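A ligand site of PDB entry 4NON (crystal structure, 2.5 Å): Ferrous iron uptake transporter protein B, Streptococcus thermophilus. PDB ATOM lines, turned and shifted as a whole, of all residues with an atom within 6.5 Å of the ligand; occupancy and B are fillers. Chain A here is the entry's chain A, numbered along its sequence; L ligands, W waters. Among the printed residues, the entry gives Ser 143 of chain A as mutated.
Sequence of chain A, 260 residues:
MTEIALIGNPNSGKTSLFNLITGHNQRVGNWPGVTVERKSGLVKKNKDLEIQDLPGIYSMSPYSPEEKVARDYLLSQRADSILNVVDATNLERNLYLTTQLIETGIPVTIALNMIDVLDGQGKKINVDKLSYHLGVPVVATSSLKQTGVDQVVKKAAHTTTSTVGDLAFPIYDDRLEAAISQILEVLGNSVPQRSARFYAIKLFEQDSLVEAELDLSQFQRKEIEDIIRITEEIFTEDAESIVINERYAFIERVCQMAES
An oxygen (O5) of the ligand is in hydrogen-bond range of the backbone NH (N) of Ser 16, 2.8 Å away. OG of Ser 16 is in hydrogen-bond range of O5 of the ligand. N of Thr 15 lies within hydrogen-bond range of O1 of the ligand (2.9 Å). An oxygen (O1) of the ligand lies within hydrogen-bond range of the side-chain hydroxyl (OG1) of Thr 15. N of Ser 143 is in hydrogen-bond range of O11 of the ligand, 2.8 Å away. N of Lys 14 lies within hydrogen-bond range of O2 of the ligand, at 2.8 Å. O3 of the ligand sits at hydrogen-bond distance from N of Asn 11, 2.8 Å away. The backbone NH (N) of Gly 13 lies within hydrogen-bond range of an oxygen (O2) of the ligand (2.9 Å). An oxygen (O2) of the ligand lies within hydrogen-bond range of the backbone NH of Ser 12, 3.1 Å away. OD1 of Asp 116 is in hydrogen-bond range of N3 of the ligand. N of Leu 144 sits at hydrogen-bond distance from O11 of the ligand (3.3 Å).
O of Gly 13 sits at hydrogen-bond distance from ND2 of Asn 113. OG of Ser 12 sits at hydrogen-bond distance from O of Asn 9, at 2.6 Å. The backbone carbonyl oxygen (O) of Ser 12 lies within hydrogen-bond range of the side-chain amide nitrogen (ND2) of Asn 113, at 3.0 Å. OD1 of Asp 116 lies within hydrogen-bond range of OG of Ser 142, 3.1 Å away. The backbone NH (N) of Leu 144 sits close to the side-chain hydroxyl (OG) of Ser 142, at 3.3 Å. N of Met 114 is in hydrogen-bond range of O of Thr 141. The backbone NH (N) of Lys 145 lies within hydrogen-bond range of the side-chain hydroxyl (OG) of Ser 142 (2.8 Å).
Asn 9 touches the ligand. Pro 10 touches the ligand. Met 114 touches the ligand. CG2 of Val 117 touches N4 of the ligand, 3.1 Å away. C of Ser 142 touches O11 of the ligand, at 3.6 Å. Hydrophobic or aromatic side chains within 4 Å of the ligand: Met 114, Val 117 and Leu 144. Of the 22 residues printed, 14 come within 4 Å of the ligand.
Water W1 lies within hydrogen-bond range of an oxygen (O2) of the ligand (2.7 Å), the backbone carbonyl oxygen of Asn 9 (3.3 Å) and the side-chain amino group of Lys 14 (3.5 Å).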
ATOM      1  N   GLY A   8      -4.926   2.807  -5.498  1.00  0.00           N
ATOM      2  CA  GLY A   8      -4.333   2.543  -4.189  1.00  0.00           C
ATOM      3  C   GLY A   8      -3.091   1.679  -4.284  1.00  0.00           C
ATOM      4  O   GLY A   8      -2.668   1.303  -5.375  1.00  0.00           O
ATOM      5  N   ASN A   9      -2.494   1.376  -3.134  1.00  0.00           N
ATOM      6  CA  ASN A   9      -1.407   0.410  -3.074  1.00  0.00           C
ATOM      7  C   ASN A   9      -1.910  -0.972  -3.468  1.00  0.00           C
ATOM      8  O   ASN A   9      -3.112  -1.254  -3.368  1.00  0.00           O
ATOM      9  CB  ASN A   9      -0.813   0.325  -1.666  1.00  0.00           C
ATOM     10  CG  ASN A   9      -0.066   1.589  -1.226  1.00  0.00           C
ATOM     11  OD1 ASN A   9       0.462   1.633  -0.118  1.00  0.00           O
ATOM     12  ND2 ASN A   9      -0.039   2.616  -2.078  1.00  0.00           N
ATOM     13  N   PRO A  10      -1.000  -1.853  -3.932  1.00  0.00           N
ATOM     14  CA  PRO A  10      -1.352  -3.261  -4.075  1.00  0.00           C
ATOM     15  C   PRO A  10      -1.742  -3.867  -2.722  1.00  0.00           C
ATOM     16  O   PRO A  10      -1.220  -3.445  -1.687  1.00  0.00           O
ATOM     17  CB  PRO A  10      -0.067  -3.896  -4.605  1.00  0.00           C
ATOM     18  CG  PRO A  10       0.636  -2.795  -5.299  1.00  0.00           C
ATOM     19  CD  PRO A  10       0.330  -1.560  -4.494  1.00  0.00           C
ATOM     20  N   ASN A  11      -2.633  -4.856  -2.762  1.00  0.00           N
ATOM     21  CA  ASN A  11      -3.147  -5.515  -1.554  1.00  0.00           C
ATOM     22  C   ASN A  11      -3.801  -4.554  -0.549  1.00  0.00           C
ATOM     23  O   ASN A  11      -3.723  -4.756   0.659  1.00  0.00           O
ATOM     24  CB  ASN A  11      -2.060  -6.375  -0.889  1.00  0.00           C
ATOM     25  CG  ASN A  11      -2.021  -7.785  -1.455  1.00  0.00           C
ATOM     26  OD1 ASN A  11      -1.806  -7.981  -2.649  1.00  0.00           O
ATOM     27  ND2 ASN A  11      -2.222  -8.780  -0.588  1.00  0.00           N
ATOM     28  N   SER A  12      -4.458  -3.523  -1.071  1.00  0.00           N
ATOM     29  CA  SER A  12      -5.295  -2.629  -0.261  1.00  0.00           C
ATOM     30  C   SER A  12      -6.781  -2.975  -0.403  1.00  0.00           C
ATOM     31  O   SER A  12      -7.613  -2.393   0.287  1.00  0.00           O
ATOM     32  CB  SER A  12      -5.048  -1.174  -0.661  1.00  0.00           C
ATOM     33  OG  SER A  12      -5.310  -0.966  -2.034  1.00  0.00           O
ATOM     34  N   GLY A  13      -7.096  -3.922  -1.283  1.00  0.00           N
ATOM     35  CA  GLY A  13      -8.483  -4.328  -1.528  1.00  0.00           C
ATOM     36  C   GLY A  13      -9.155  -3.547  -2.636  1.00  0.00           C
ATOM     37  O   GLY A  13     -10.373  -3.321  -2.597  1.00  0.00           O
ATOM     38  N   LYS A  14      -8.378  -3.123  -3.636  1.00  0.00           N
ATOM     39  CA  LYS A  14      -8.928  -2.334  -4.743  1.00  0.00           C
ATOM     40  C   LYS A  14      -9.812  -3.167  -5.669  1.00  0.00           C
ATOM     41  O   LYS A  14     -10.893  -2.717  -6.058  1.00  0.00           O
ATOM     42  CB  LYS A  14      -7.810  -1.665  -5.559  1.00  0.00           C
ATOM     43  CG  LYS A  14      -8.326  -0.709  -6.622  1.00  0.00           C
ATOM     44  CD  LYS A  14      -7.335   0.393  -6.976  1.00  0.00           C
ATOM     45  CE  LYS A  14      -6.015  -0.147  -7.491  1.00  0.00           C
ATOM     46  NZ  LYS A  14      -6.187  -1.167  -8.571  1.00  0.00           N
ATOM     47  N   THR A  15      -9.370  -4.372  -6.004  1.00  0.00           N
ATOM     48  CA  THR A  15     -10.120  -5.257  -6.891  1.00  0.00           C
ATOM     49  C   THR A  15     -11.431  -5.711  -6.246  1.00  0.00           C
ATOM     50  O   THR A  15     -12.488  -5.706  -6.883  1.00  0.00           O
ATOM     51  CB  THR A  15      -9.291  -6.491  -7.297  1.00  0.00           C
ATOM     52  OG1 THR A  15      -8.060  -6.063  -7.889  1.00  0.00           O
ATOM     53  CG2 THR A  15     -10.061  -7.357  -8.283  1.00  0.00           C
ATOM     54  N   SER A  16     -11.354  -6.130  -4.986  1.00  0.00           N
ATOM     55  CA  SER A  16     -12.522  -6.593  -4.232  1.00  0.00           C
ATOM     56  C   SER A  16     -13.598  -5.508  -4.185  1.00  0.00           C
ATOM     57  O   SER A  16     -14.777  -5.789  -4.397  1.00  0.00           O
ATOM     58  CB  SER A  16     -12.124  -6.942  -2.801  1.00  0.00           C
ATOM     59  OG  SER A  16     -10.947  -7.738  -2.780  1.00  0.00           O
ATOM     60  N   LEU A  17     -13.164  -4.288  -3.906  1.00  0.00           N
ATOM     61  CA  LEU A  17     -14.054  -3.140  -3.813  1.00  0.00           C
ATOM     62  C   LEU A  17     -14.587  -2.761  -5.190  1.00  0.00           C
ATOM     63  O   LEU A  17     -15.775  -2.463  -5.340  1.00  0.00           O
ATOM     64  CB  LEU A  17     -13.296  -1.964  -3.185  1.00  0.00           C
ATOM     65  CG  LEU A  17     -14.071  -0.749  -2.663  1.00  0.00           C
ATOM     66  CD1 LEU A  17     -15.163  -1.143  -1.689  1.00  0.00           C
ATOM     67  CD2 LEU A  17     -13.083   0.207  -1.998  1.00  0.00           C
ATOM     68  N   LYS A  39      -8.910  -1.886 -16.502  1.00  0.00           N
ATOM     69  CA  LYS A  39     -10.285  -2.243 -16.157  1.00  0.00           C
ATOM     70  C   LYS A  39     -11.131  -0.981 -15.991  1.00  0.00           C
ATOM     71  O   LYS A  39     -10.670  -0.002 -15.412  1.00  0.00           O
ATOM     72  CB  LYS A  39     -10.342  -3.051 -14.863  1.00  0.00           C
ATOM     73  CG  LYS A  39      -9.505  -4.326 -14.862  1.00  0.00           C
ATOM     74  CD  LYS A  39      -9.761  -5.179 -13.618  1.00  0.00           C
ATOM     75  CE  LYS A  39      -9.361  -4.463 -12.332  1.00  0.00           C
ATOM     76  NZ  LYS A  39      -9.439  -5.348 -11.137  1.00  0.00           N
ATOM     77  N   VAL A  85      -8.263   4.092  -2.350  1.00  0.00           N
ATOM     78  CA  VAL A  85      -8.423   2.944  -1.448  1.00  0.00           C
ATOM     79  C   VAL A  85      -7.196   2.810  -0.559  1.00  0.00           C
ATOM     80  O   VAL A  85      -6.103   2.516  -1.025  1.00  0.00           O
ATOM     81  CB  VAL A  85      -8.616   1.622  -2.231  1.00  0.00           C
ATOM     82  CG1 VAL A  85      -8.741   0.448  -1.262  1.00  0.00           C
ATOM     83  CG2 VAL A  85      -9.841   1.712  -3.127  1.00  0.00           C
ATOM     84  N   ASN A 113     -10.118   1.199   3.894  1.00  0.00           N
ATOM     85  CA  ASN A 113     -10.570  -0.159   3.622  1.00  0.00           C
ATOM     86  C   ASN A 113     -10.066  -1.194   4.639  1.00  0.00           C
ATOM     87  O   ASN A 113      -9.124  -0.929   5.384  1.00  0.00           O
ATOM     88  CB  ASN A 113     -10.156  -0.556   2.198  1.00  0.00           C
ATOM     89  CG  ASN A 113     -11.066  -1.602   1.583  1.00  0.00           C
ATOM     90  OD1 ASN A 113     -12.186  -1.821   2.044  1.00  0.00           O
ATOM     91  ND2 ASN A 113     -10.595  -2.238   0.518  1.00  0.00           N
ATOM     92  N   MET A 114     -10.709  -2.357   4.640  1.00  0.00           N
ATOM     93  CA  MET A 114     -10.364  -3.465   5.535  1.00  0.00           C
ATOM     94  C   MET A 114     -10.470  -3.023   6.992  1.00  0.00           C
ATOM     95  O   MET A 114      -9.606  -3.336   7.816  1.00  0.00           O
ATOM     96  CB  MET A 114      -8.966  -3.992   5.228  1.00  0.00           C
ATOM     97  CG  MET A 114      -8.787  -4.431   3.780  1.00  0.00           C
ATOM     98  SD  MET A 114      -7.118  -5.007   3.426  1.00  0.00           S
ATOM     99  CE  MET A 114      -7.322  -5.612   1.763  1.00  0.00           C
ATOM    100  N   ILE A 115     -11.537  -2.296   7.308  1.00  0.00           N
ATOM    101  CA  ILE A 115     -11.745  -1.747   8.649  1.00  0.00           C
ATOM    102  C   ILE A 115     -12.107  -2.840   9.649  1.00  0.00           C
ATOM    103  O   ILE A 115     -11.795  -2.717  10.839  1.00  0.00           O
ATOM    104  CB  ILE A 115     -12.816  -0.628   8.631  1.00  0.00           C
ATOM    105  CG1 ILE A 115     -12.771   0.197   9.924  1.00  0.00           C
ATOM    106  CG2 ILE A 115     -14.217  -1.188   8.408  1.00  0.00           C
ATOM    107  CD1 ILE A 115     -11.495   1.008  10.093  1.00  0.00           C
ATOM    108  N   ASP A 116     -12.744  -3.909   9.170  1.00  0.00           N
ATOM    109  CA  ASP A 116     -13.018  -5.084  10.003  1.00  0.00           C
ATOM    110  C   ASP A 116     -11.732  -5.754  10.508  1.00  0.00           C
ATOM    111  O   ASP A 116     -11.716  -6.309  11.599  1.00  0.00           O
ATOM    112  CB  ASP A 116     -13.882  -6.112   9.257  1.00  0.00           C
ATOM    113  CG  ASP A 116     -13.165  -6.715   8.047  1.00  0.00           C
ATOM    114  OD1 ASP A 116     -12.889  -5.972   7.082  1.00  0.00           O
ATOM    115  OD2 ASP A 116     -12.881  -7.926   8.069  1.00  0.00           O
ATOM    116  N   VAL A 117     -10.672  -5.693   9.704  1.00  0.00           N
ATOM    117  CA  VAL A 117      -9.387  -6.287  10.077  1.00  0.00           C
ATOM    118  C   VAL A 117      -8.725  -5.467  11.170  1.00  0.00           C
ATOM    119  O   VAL A 117      -8.064  -6.024  12.054  1.00  0.00           O
ATOM    120  CB  VAL A 117      -8.427  -6.400   8.867  1.00  0.00           C
ATOM    121  CG1 VAL A 117      -7.156  -7.139   9.259  1.00  0.00           C
ATOM    122  CG2 VAL A 117      -9.101  -7.107   7.706  1.00  0.00           C
ATOM    123  N   THR A 141     -14.552   1.423   5.085  1.00  0.00           N
ATOM    124  CA  THR A 141     -15.106   0.408   4.201  1.00  0.00           C
ATOM    125  C   THR A 141     -14.587  -0.993   4.518  1.00  0.00           C
ATOM    126  O   THR A 141     -13.457  -1.161   4.974  1.00  0.00           O
ATOM    127  CB  THR A 141     -14.825   0.715   2.721  1.00  0.00           C
ATOM    128  OG1 THR A 141     -13.421   0.692   2.467  1.00  0.00           O
ATOM    129  CG2 THR A 141     -15.373   2.083   2.345  1.00  0.00           C
ATOM    130  N   SER A 142     -15.451  -1.984   4.292  1.00  0.00           N
ATOM    131  CA  SER A 142     -15.064  -3.379   4.286  1.00  0.00           C
ATOM    132  C   SER A 142     -15.711  -4.035   3.072  1.00  0.00           C
ATOM    133  O   SER A 142     -16.934  -3.962   2.896  1.00  0.00           O
ATOM    134  CB  SER A 142     -15.521  -4.082   5.564  1.00  0.00           C
ATOM    135  OG  SER A 142     -15.495  -5.499   5.419  1.00  0.00           O
ATOM    136  N   SER A 143     -14.896  -4.648   2.223  1.00  0.00           N
ATOM    137  CA  SER A 143     -15.390  -5.400   1.071  1.00  0.00           C
ATOM    138  C   SER A 143     -15.995  -6.731   1.528  1.00  0.00           C
ATOM    139  O   SER A 143     -16.924  -7.245   0.896  1.00  0.00           O
ATOM    140  CB  SER A 143     -14.255  -5.650   0.082  1.00  0.00           C
ATOM    141  OG  SER A 143     -13.470  -4.489  -0.089  1.00  0.00           O
ATOM    142  N   LEU A 144     -15.459  -7.285   2.613  1.00  0.00           N
ATOM    143  CA  LEU A 144     -15.957  -8.543   3.188  1.00  0.00           C
ATOM    144  C   LEU A 144     -17.335  -8.365   3.823  1.00  0.00           C
ATOM    145  O   LEU A 144     -18.281  -9.062   3.458  1.00  0.00           O
ATOM    146  CB  LEU A 144     -14.972  -9.077   4.228  1.00  0.00           C
ATOM    147  CG  LEU A 144     -15.380 -10.330   5.012  1.00  0.00           C
ATOM    148  CD1 LEU A 144     -15.681 -11.478   4.059  1.00  0.00           C
ATOM    149  CD2 LEU A 144     -14.287 -10.709   5.994  1.00  0.00           C
ATOM    150  N   LYS A 145     -17.438  -7.429   4.761  1.00  0.00           N
ATOM    151  CA  LYS A 145     -18.699  -7.172   5.457  1.00  0.00           C
ATOM    152  C   LYS A 145     -19.680  -6.335   4.635  1.00  0.00           C
ATOM    153  O   LYS A 145     -20.836  -6.192   5.023  1.00  0.00           O
ATOM    154  CB  LYS A 145     -18.456  -6.499   6.814  1.00  0.00           C
ATOM    155  CG  LYS A 145     -17.513  -7.242   7.750  1.00  0.00           C
ATOM    156  CD  LYS A 145     -17.977  -8.670   8.036  1.00  0.00           C
ATOM    157  CE  LYS A 145     -17.057  -9.353   9.040  1.00  0.00           C
ATOM    158  NZ  LYS A 145     -17.309 -10.820   9.136  1.00  0.00           N
HETATM  159  P1  LIG L   1      -5.810  -5.412  -4.470  1.00  0.00           P
HETATM  160  O1  LIG L   1      -6.689  -5.519  -5.683  1.00  0.00           O
HETATM  161  O2  LIG L   1      -5.780  -4.042  -3.827  1.00  0.00           O
HETATM  162  O3  LIG L   1      -4.430  -6.032  -4.593  1.00  0.00           O
HETATM  163  O4  LIG L   1      -6.531  -6.291  -3.326  1.00  0.00           O
HETATM  164  P2  LIG L   1      -7.526  -7.517  -3.600  1.00  0.00           P
HETATM  165  O5  LIG L   1      -8.893  -6.972  -3.891  1.00  0.00           O
HETATM  166  O6  LIG L   1      -6.884  -8.489  -4.568  1.00  0.00           O
HETATM  167  O7  LIG L   1      -7.543  -8.207  -2.149  1.00  0.00           O
HETATM  168  C1  LIG L   1      -6.325  -8.377  -1.439  1.00  0.00           C
HETATM  169  C2  LIG L   1      -6.480  -9.422  -0.348  1.00  0.00           C
HETATM  170  O8  LIG L   1      -7.161  -8.843   0.768  1.00  0.00           O
HETATM  171  C3  LIG L   1      -7.289 -10.637  -0.773  1.00  0.00           C
HETATM  172  O9  LIG L   1      -6.635 -11.848  -0.350  1.00  0.00           O
HETATM  173  C4  LIG L   1      -8.638 -10.486  -0.102  1.00  0.00           C
HETATM  174  O10 LIG L   1      -9.123 -11.740   0.374  1.00  0.00           O
HETATM  175  C5  LIG L   1      -8.375  -9.535   1.051  1.00  0.00           C
HETATM  176  N1  LIG L   1      -9.426  -8.510   1.264  1.00  0.00           N
HETATM  177  C6  LIG L   1      -9.886  -7.612   0.362  1.00  0.00           C
HETATM  178  N2  LIG L   1     -10.826  -6.805   0.908  1.00  0.00           N
HETATM  179  C7  LIG L   1     -10.983  -7.174   2.198  1.00  0.00           C
HETATM  180  C8  LIG L   1     -11.807  -6.754   3.348  1.00  0.00           C
HETATM  181  O11 LIG L   1     -12.615  -5.805   3.239  1.00  0.00           O
HETATM  182  N3  LIG L   1     -11.658  -7.394   4.510  1.00  0.00           N
HETATM  183  C9  LIG L   1     -10.786  -8.417   4.655  1.00  0.00           C
HETATM  184  N4  LIG L   1     -10.681  -9.039   5.862  1.00  0.00           N
HETATM  185  N5  LIG L   1     -10.004  -8.862   3.649  1.00  0.00           N
HETATM  186  C10 LIG L   1     -10.048  -8.292   2.418  1.00  0.00           C
HETATM  187  O   HOH W   1      -4.628  -2.691  -5.890  1.00  0.00           O
